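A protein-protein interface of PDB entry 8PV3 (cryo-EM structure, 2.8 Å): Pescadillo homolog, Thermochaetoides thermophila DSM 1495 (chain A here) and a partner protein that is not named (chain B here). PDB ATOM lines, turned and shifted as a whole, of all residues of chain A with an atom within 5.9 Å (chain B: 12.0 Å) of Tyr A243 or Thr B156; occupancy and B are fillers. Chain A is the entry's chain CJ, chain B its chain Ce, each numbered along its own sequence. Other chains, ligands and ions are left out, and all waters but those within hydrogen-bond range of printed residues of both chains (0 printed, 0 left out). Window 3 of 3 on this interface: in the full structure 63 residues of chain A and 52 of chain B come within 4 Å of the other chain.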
ATOM      1  N   LEU A 238       3.711  11.785 -16.904  1.00  0.00           N
ATOM      2  CA  LEU A 238       3.278  13.094 -16.428  1.00  0.00           C
ATOM      3  C   LEU A 238       2.150  13.661 -17.275  1.00  0.00           C
ATOM      4  O   LEU A 238       1.324  14.419 -16.758  1.00  0.00           O
ATOM      5  CB  LEU A 238       4.458  14.069 -16.386  1.00  0.00           C
ATOM      6  CG  LEU A 238       4.179  15.399 -15.672  1.00  0.00           C
ATOM      7  CD1 LEU A 238       3.614  15.152 -14.282  1.00  0.00           C
ATOM      8  CD2 LEU A 238       5.407  16.282 -15.595  1.00  0.00           C
ATOM      9  N   GLY A 239       2.076  13.294 -18.559  1.00  0.00           N
ATOM     10  CA  GLY A 239       0.926  13.702 -19.357  1.00  0.00           C
ATOM     11  C   GLY A 239      -0.393  13.187 -18.803  1.00  0.00           C
ATOM     12  O   GLY A 239      -1.353  13.950 -18.635  1.00  0.00           O
ATOM     13  N   PHE A 240      -0.442  11.897 -18.460  1.00  0.00           N
ATOM     14  CA  PHE A 240      -1.657  11.317 -17.896  1.00  0.00           C
ATOM     15  C   PHE A 240      -1.934  11.846 -16.495  1.00  0.00           C
ATOM     16  O   PHE A 240      -3.099  12.056 -16.128  1.00  0.00           O
ATOM     17  CB  PHE A 240      -1.551   9.795 -17.884  1.00  0.00           C
ATOM     18  CG  PHE A 240      -1.592   9.179 -19.249  1.00  0.00           C
ATOM     19  CD1 PHE A 240      -2.538   9.585 -20.172  1.00  0.00           C
ATOM     20  CD2 PHE A 240      -0.692   8.193 -19.609  1.00  0.00           C
ATOM     21  CE1 PHE A 240      -2.583   9.026 -21.428  1.00  0.00           C
ATOM     22  CE2 PHE A 240      -0.734   7.628 -20.864  1.00  0.00           C
ATOM     23  CZ  PHE A 240      -1.683   8.046 -21.773  1.00  0.00           C
ATOM     24  N   VAL A 241      -0.881  12.065 -15.698  1.00  0.00           N
ATOM     25  CA  VAL A 241      -1.070  12.626 -14.360  1.00  0.00           C
ATOM     26  C   VAL A 241      -1.665  14.028 -14.446  1.00  0.00           C
ATOM     27  O   VAL A 241      -2.605  14.366 -13.711  1.00  0.00           O
ATOM     28  CB  VAL A 241       0.259  12.618 -13.581  1.00  0.00           C
ATOM     29  CG1 VAL A 241       0.137  13.420 -12.300  1.00  0.00           C
ATOM     30  CG2 VAL A 241       0.670  11.197 -13.258  1.00  0.00           C
ATOM     31  N   ASN A 242      -1.157  14.847 -15.370  1.00  0.00           N
ATOM     32  CA  ASN A 242      -1.685  16.193 -15.560  1.00  0.00           C
ATOM     33  C   ASN A 242      -3.127  16.162 -16.042  1.00  0.00           C
ATOM     34  O   ASN A 242      -3.948  16.970 -15.592  1.00  0.00           O
ATOM     35  CB  ASN A 242      -0.813  16.963 -16.548  1.00  0.00           C
ATOM     36  CG  ASN A 242       0.452  17.491 -15.918  1.00  0.00           C
ATOM     37  OD1 ASN A 242       0.595  17.500 -14.696  1.00  0.00           O
ATOM     38  ND2 ASN A 242       1.382  17.942 -16.749  1.00  0.00           N
ATOM     39  N   TYR A 243      -3.454  15.242 -16.958  1.00  0.00           N
ATOM     40  CA  TYR A 243      -4.834  15.142 -17.432  1.00  0.00           C
ATOM     41  C   TYR A 243      -5.780  14.773 -16.298  1.00  0.00           C
ATOM     42  O   TYR A 243      -6.861  15.361 -16.164  1.00  0.00           O
ATOM     43  CB  TYR A 243      -4.947  14.122 -18.564  1.00  0.00           C
ATOM     44  CG  TYR A 243      -6.377  13.901 -19.007  1.00  0.00           C
ATOM     45  CD1 TYR A 243      -7.024  14.831 -19.809  1.00  0.00           C
ATOM     46  CD2 TYR A 243      -7.080  12.764 -18.626  1.00  0.00           C
ATOM     47  CE1 TYR A 243      -8.329  14.640 -20.214  1.00  0.00           C
ATOM     48  CE2 TYR A 243      -8.387  12.567 -19.026  1.00  0.00           C
ATOM     49  CZ  TYR A 243      -9.005  13.507 -19.820  1.00  0.00           C
ATOM     50  OH  TYR A 243     -10.305  13.316 -20.226  1.00  0.00           O
ATOM     51  N   ARG A 244      -5.380  13.813 -15.460  1.00  0.00           N
ATOM     52  CA  ARG A 244      -6.244  13.398 -14.361  1.00  0.00           C
ATOM     53  C   ARG A 244      -6.417  14.510 -13.336  1.00  0.00           C
ATOM     54  O   ARG A 244      -7.523  14.723 -12.830  1.00  0.00           O
ATOM     55  CB  ARG A 244      -5.700  12.137 -13.695  1.00  0.00           C
ATOM     56  CG  ARG A 244      -6.634  11.585 -12.633  1.00  0.00           C
ATOM     57  CD  ARG A 244      -6.210  10.214 -12.160  1.00  0.00           C
ATOM     58  NE  ARG A 244      -7.025   9.757 -11.041  1.00  0.00           N
ATOM     59  CZ  ARG A 244      -8.189   9.138 -11.167  1.00  0.00           C
ATOM     60  NH1 ARG A 244      -8.708   8.880 -12.356  1.00  0.00           N
ATOM     61  NH2 ARG A 244      -8.848   8.767 -10.074  1.00  0.00           N
ATOM     62  N   LEU A 245      -5.347  15.252 -13.038  1.00  0.00           N
ATOM     63  CA  LEU A 245      -5.454  16.337 -12.063  1.00  0.00           C
ATOM     64  C   LEU A 245      -6.320  17.484 -12.582  1.00  0.00           C
ATOM     65  O   LEU A 245      -7.161  18.020 -11.841  1.00  0.00           O
ATOM     66  CB  LEU A 245      -4.060  16.836 -11.688  1.00  0.00           C
ATOM     67  CG  LEU A 245      -3.207  15.856 -10.879  1.00  0.00           C
ATOM     68  CD1 LEU A 245      -1.803  16.394 -10.684  1.00  0.00           C
ATOM     69  CD2 LEU A 245      -3.854  15.553  -9.543  1.00  0.00           C
ATOM     70  N   TYR A 246      -6.140  17.868 -13.850  1.00  0.00           N
ATOM     71  CA  TYR A 246      -6.950  18.937 -14.424  1.00  0.00           C
ATOM     72  C   TYR A 246      -8.417  18.535 -14.520  1.00  0.00           C
ATOM     73  O   TYR A 246      -9.305  19.352 -14.254  1.00  0.00           O
ATOM     74  CB  TYR A 246      -6.411  19.332 -15.798  1.00  0.00           C
ATOM     75  CG  TYR A 246      -5.290  20.346 -15.759  1.00  0.00           C
ATOM     76  CD1 TYR A 246      -4.089  20.061 -15.127  1.00  0.00           C
ATOM     77  CD2 TYR A 246      -5.434  21.589 -16.358  1.00  0.00           C
ATOM     78  CE1 TYR A 246      -3.063  20.980 -15.094  1.00  0.00           C
ATOM     79  CE2 TYR A 246      -4.414  22.515 -16.326  1.00  0.00           C
ATOM     80  CZ  TYR A 246      -3.231  22.204 -15.694  1.00  0.00           C
ATOM     81  OH  TYR A 246      -2.209  23.122 -15.659  1.00  0.00           O
ATOM     82  N   THR A 247      -8.695  17.280 -14.888  1.00  0.00           N
ATOM     83  CA  THR A 247     -10.079  16.820 -14.922  1.00  0.00           C
ATOM     84  C   THR A 247     -10.671  16.719 -13.520  1.00  0.00           C
ATOM     85  O   THR A 247     -11.869  16.962 -13.337  1.00  0.00           O
ATOM     86  CB  THR A 247     -10.162  15.474 -15.642  1.00  0.00           C
ATOM     87  OG1 THR A 247      -9.387  15.533 -16.844  1.00  0.00           O
ATOM     88  CG2 THR A 247     -11.601  15.143 -16.004  1.00  0.00           C
ATOM     89  N   SER A 248      -9.850  16.378 -12.523  1.00  0.00           N
ATOM     90  CA  SER A 248     -10.329  16.308 -11.148  1.00  0.00           C
ATOM     91  C   SER A 248     -10.695  17.681 -10.608  1.00  0.00           C
ATOM     92  O   SER A 248     -11.656  17.804  -9.841  1.00  0.00           O
ATOM     93  CB  SER A 248      -9.274  15.656 -10.256  1.00  0.00           C
ATOM     94  OG  SER A 248      -8.207  16.550  -9.994  1.00  0.00           O
ATOM     95  N   TYR A 253      -8.055  20.230 -20.300  1.00  0.00           N
ATOM     96  CA  TYR A 253      -6.702  19.765 -20.556  1.00  0.00           C
ATOM     97  C   TYR A 253      -6.602  19.342 -22.016  1.00  0.00           C
ATOM     98  O   TYR A 253      -7.484  18.620 -22.513  1.00  0.00           O
ATOM     99  CB  TYR A 253      -6.317  18.601 -19.635  1.00  0.00           C
ATOM    100  CG  TYR A 253      -4.861  18.210 -19.750  1.00  0.00           C
ATOM    101  CD1 TYR A 253      -3.874  18.936 -19.097  1.00  0.00           C
ATOM    102  CD2 TYR A 253      -4.472  17.124 -20.520  1.00  0.00           C
ATOM    103  CE1 TYR A 253      -2.544  18.589 -19.206  1.00  0.00           C
ATOM    104  CE2 TYR A 253      -3.144  16.768 -20.633  1.00  0.00           C
ATOM    105  CZ  TYR A 253      -2.186  17.502 -19.974  1.00  0.00           C
ATOM    106  OH  TYR A 253      -0.863  17.150 -20.086  1.00  0.00           O
ATOM    107  N   THR B 156      -9.040  11.157 -26.468  1.00  0.00           N
ATOM    108  CA  THR B 156      -8.009  11.017 -25.446  1.00  0.00           C
ATOM    109  C   THR B 156      -8.076   9.644 -24.785  1.00  0.00           C
ATOM    110  O   THR B 156      -8.953   8.838 -25.093  1.00  0.00           O
ATOM    111  CB  THR B 156      -8.135  12.109 -24.366  1.00  0.00           C
ATOM    112  OG1 THR B 156      -6.993  12.065 -23.502  1.00  0.00           O
ATOM    113  CG2 THR B 156      -9.400  11.909 -23.545  1.00  0.00           C
ATOM    114  N   TYR B 157      -7.142   9.386 -23.874  1.00  0.00           N
ATOM    115  CA  TYR B 157      -7.071   8.108 -23.180  1.00  0.00           C
ATOM    116  C   TYR B 157      -6.699   8.384 -21.732  1.00  0.00           C
ATOM    117  O   TYR B 157      -5.797   9.178 -21.454  1.00  0.00           O
ATOM    118  CB  TYR B 157      -6.044   7.176 -23.837  1.00  0.00           C
ATOM    119  CG  TYR B 157      -5.686   5.944 -23.034  1.00  0.00           C
ATOM    120  CD1 TYR B 157      -6.671   5.094 -22.547  1.00  0.00           C
ATOM    121  CD2 TYR B 157      -4.359   5.629 -22.768  1.00  0.00           C
ATOM    122  CE1 TYR B 157      -6.345   3.966 -21.815  1.00  0.00           C
ATOM    123  CE2 TYR B 157      -4.024   4.505 -22.039  1.00  0.00           C
ATOM    124  CZ  TYR B 157      -5.019   3.677 -21.566  1.00  0.00           C
ATOM    125  OH  TYR B 157      -4.686   2.558 -20.838  1.00  0.00           O
ATOM    126  N   ASP B 158      -7.407   7.727 -20.814  1.00  0.00           N
ATOM    127  CA  ASP B 158      -7.202   7.914 -19.379  1.00  0.00           C
ATOM    128  C   ASP B 158      -7.003   6.565 -18.704  1.00  0.00           C
ATOM    129  O   ASP B 158      -7.943   5.766 -18.594  1.00  0.00           O
ATOM    130  CB  ASP B 158      -8.373   8.662 -18.747  1.00  0.00           C
ATOM    131  CG  ASP B 158      -8.113   9.033 -17.302  1.00  0.00           C
ATOM    132  OD1 ASP B 158      -6.982   9.463 -16.992  1.00  0.00           O
ATOM    133  OD2 ASP B 158      -9.035   8.889 -16.473  1.00  0.00           O
ATOM    134  N   PRO B 159      -5.787   6.274 -18.237  1.00  0.00           N
ATOM    135  CA  PRO B 159      -5.589   5.093 -17.390  1.00  0.00           C
ATOM    136  C   PRO B 159      -6.171   5.303 -16.002  1.00  0.00           C
ATOM    137  O   PRO B 159      -6.647   6.398 -15.687  1.00  0.00           O
ATOM    138  CB  PRO B 159      -4.064   4.944 -17.349  1.00  0.00           C
ATOM    139  CG  PRO B 159      -3.556   6.317 -17.605  1.00  0.00           C
ATOM    140  CD  PRO B 159      -4.511   6.917 -18.589  1.00  0.00           C
ATOM    141  N   TRP B 160      -6.146   4.259 -15.173  1.00  0.00           N
ATOM    142  CA  TRP B 160      -6.653   4.216 -13.802  1.00  0.00           C
ATOM    143  C   TRP B 160      -8.150   4.498 -13.739  1.00  0.00           C
ATOM    144  O   TRP B 160      -8.626   4.979 -12.704  1.00  0.00           O
ATOM    145  CB  TRP B 160      -5.929   5.187 -12.855  1.00  0.00           C
ATOM    146  CG  TRP B 160      -4.452   5.243 -13.061  1.00  0.00           C
ATOM    147  CD1 TRP B 160      -3.562   4.227 -12.889  1.00  0.00           C
ATOM    148  CD2 TRP B 160      -3.688   6.379 -13.479  1.00  0.00           C
ATOM    149  NE1 TRP B 160      -2.289   4.657 -13.173  1.00  0.00           N
ATOM    150  CE2 TRP B 160      -2.340   5.976 -13.537  1.00  0.00           C
ATOM    151  CE3 TRP B 160      -4.013   7.696 -13.809  1.00  0.00           C
ATOM    152  CZ2 TRP B 160      -1.320   6.843 -13.912  1.00  0.00           C
ATOM    153  CZ3 TRP B 160      -3.000   8.554 -14.181  1.00  0.00           C
ATOM    154  CH2 TRP B 160      -1.670   8.125 -14.229  1.00  0.00           C
ATOM    155  N   ALA B 161      -8.907   4.222 -14.796  1.00  0.00           N
ATOM    156  CA  ALA B 161     -10.342   4.473 -14.798  1.00  0.00           C
ATOM    157  C   ALA B 161     -11.104   3.259 -15.315  1.00  0.00           C
ATOM    158  O   ALA B 161     -10.694   2.623 -16.285  1.00  0.00           O
ATOM    159  CB  ALA B 161     -10.663   5.698 -15.637  1.00  0.00           C
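O of Tyr A243 sits at hydrogen-bond distance from OG1 of Thr A247, at 2.6 Å.
The backbone carbonyl oxygen (O) of Arg A244 lies close to the side-chain hydroxyl (OG) of Ser A248.
CE1 of Phe A240 touches O of Tyr B157 (3.2 Å).
CD of Pro B159 touches CD1 of Phe A240 (3.7 Å).
Trp B160 touches Val A241 (CH2 to CG2, 3.98 Å).
CG2 of Thr B156 touches OH of Tyr A243, 3.7 Å away.
Asp B158 touches Tyr A243 (OD1 to CD2, 3.7 Å).
Trp B160 touches Arg A244 (CE3 to CD, 3.7 Å).
Leu A238 touches none of the printed residues of chain B.
Printed residues of chain B within 4 Å of Val A241: Trp B160 (3.98 Å).
Printed residues of chain B within 4 Å of Arg A244: Trp B160 (3.7 Å).
No residue of chain B comes within 4 Å of Leu A245.
No residue of chain B comes within 4 Å of Tyr A253.
Thr B156 touches one residue of chain A.
Of the printed residues of chain A, Tyr B157 touches Phe A240 (3.2 Å).
Of the printed residues of chain A, Asp B158 touches Tyr A243.
Ala B161 touches none of the printed residues of chain A.
The nearest residue of chain A that does not touch Thr B156 is Phe A240 (5.7 Å).
Of the 6 printed residues of chain B, 5 touch a printed residue of chain A.
Along chain B the printed residues that touch a printed residue of chain A span positions 156 to 160.
Among the printed residues, 6 pairs touch across the chains.
Among the printed residues, no Asp or Glu carboxylate lies within 4 Å of a Lys or Arg side-chain nitrogen of the other chain.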
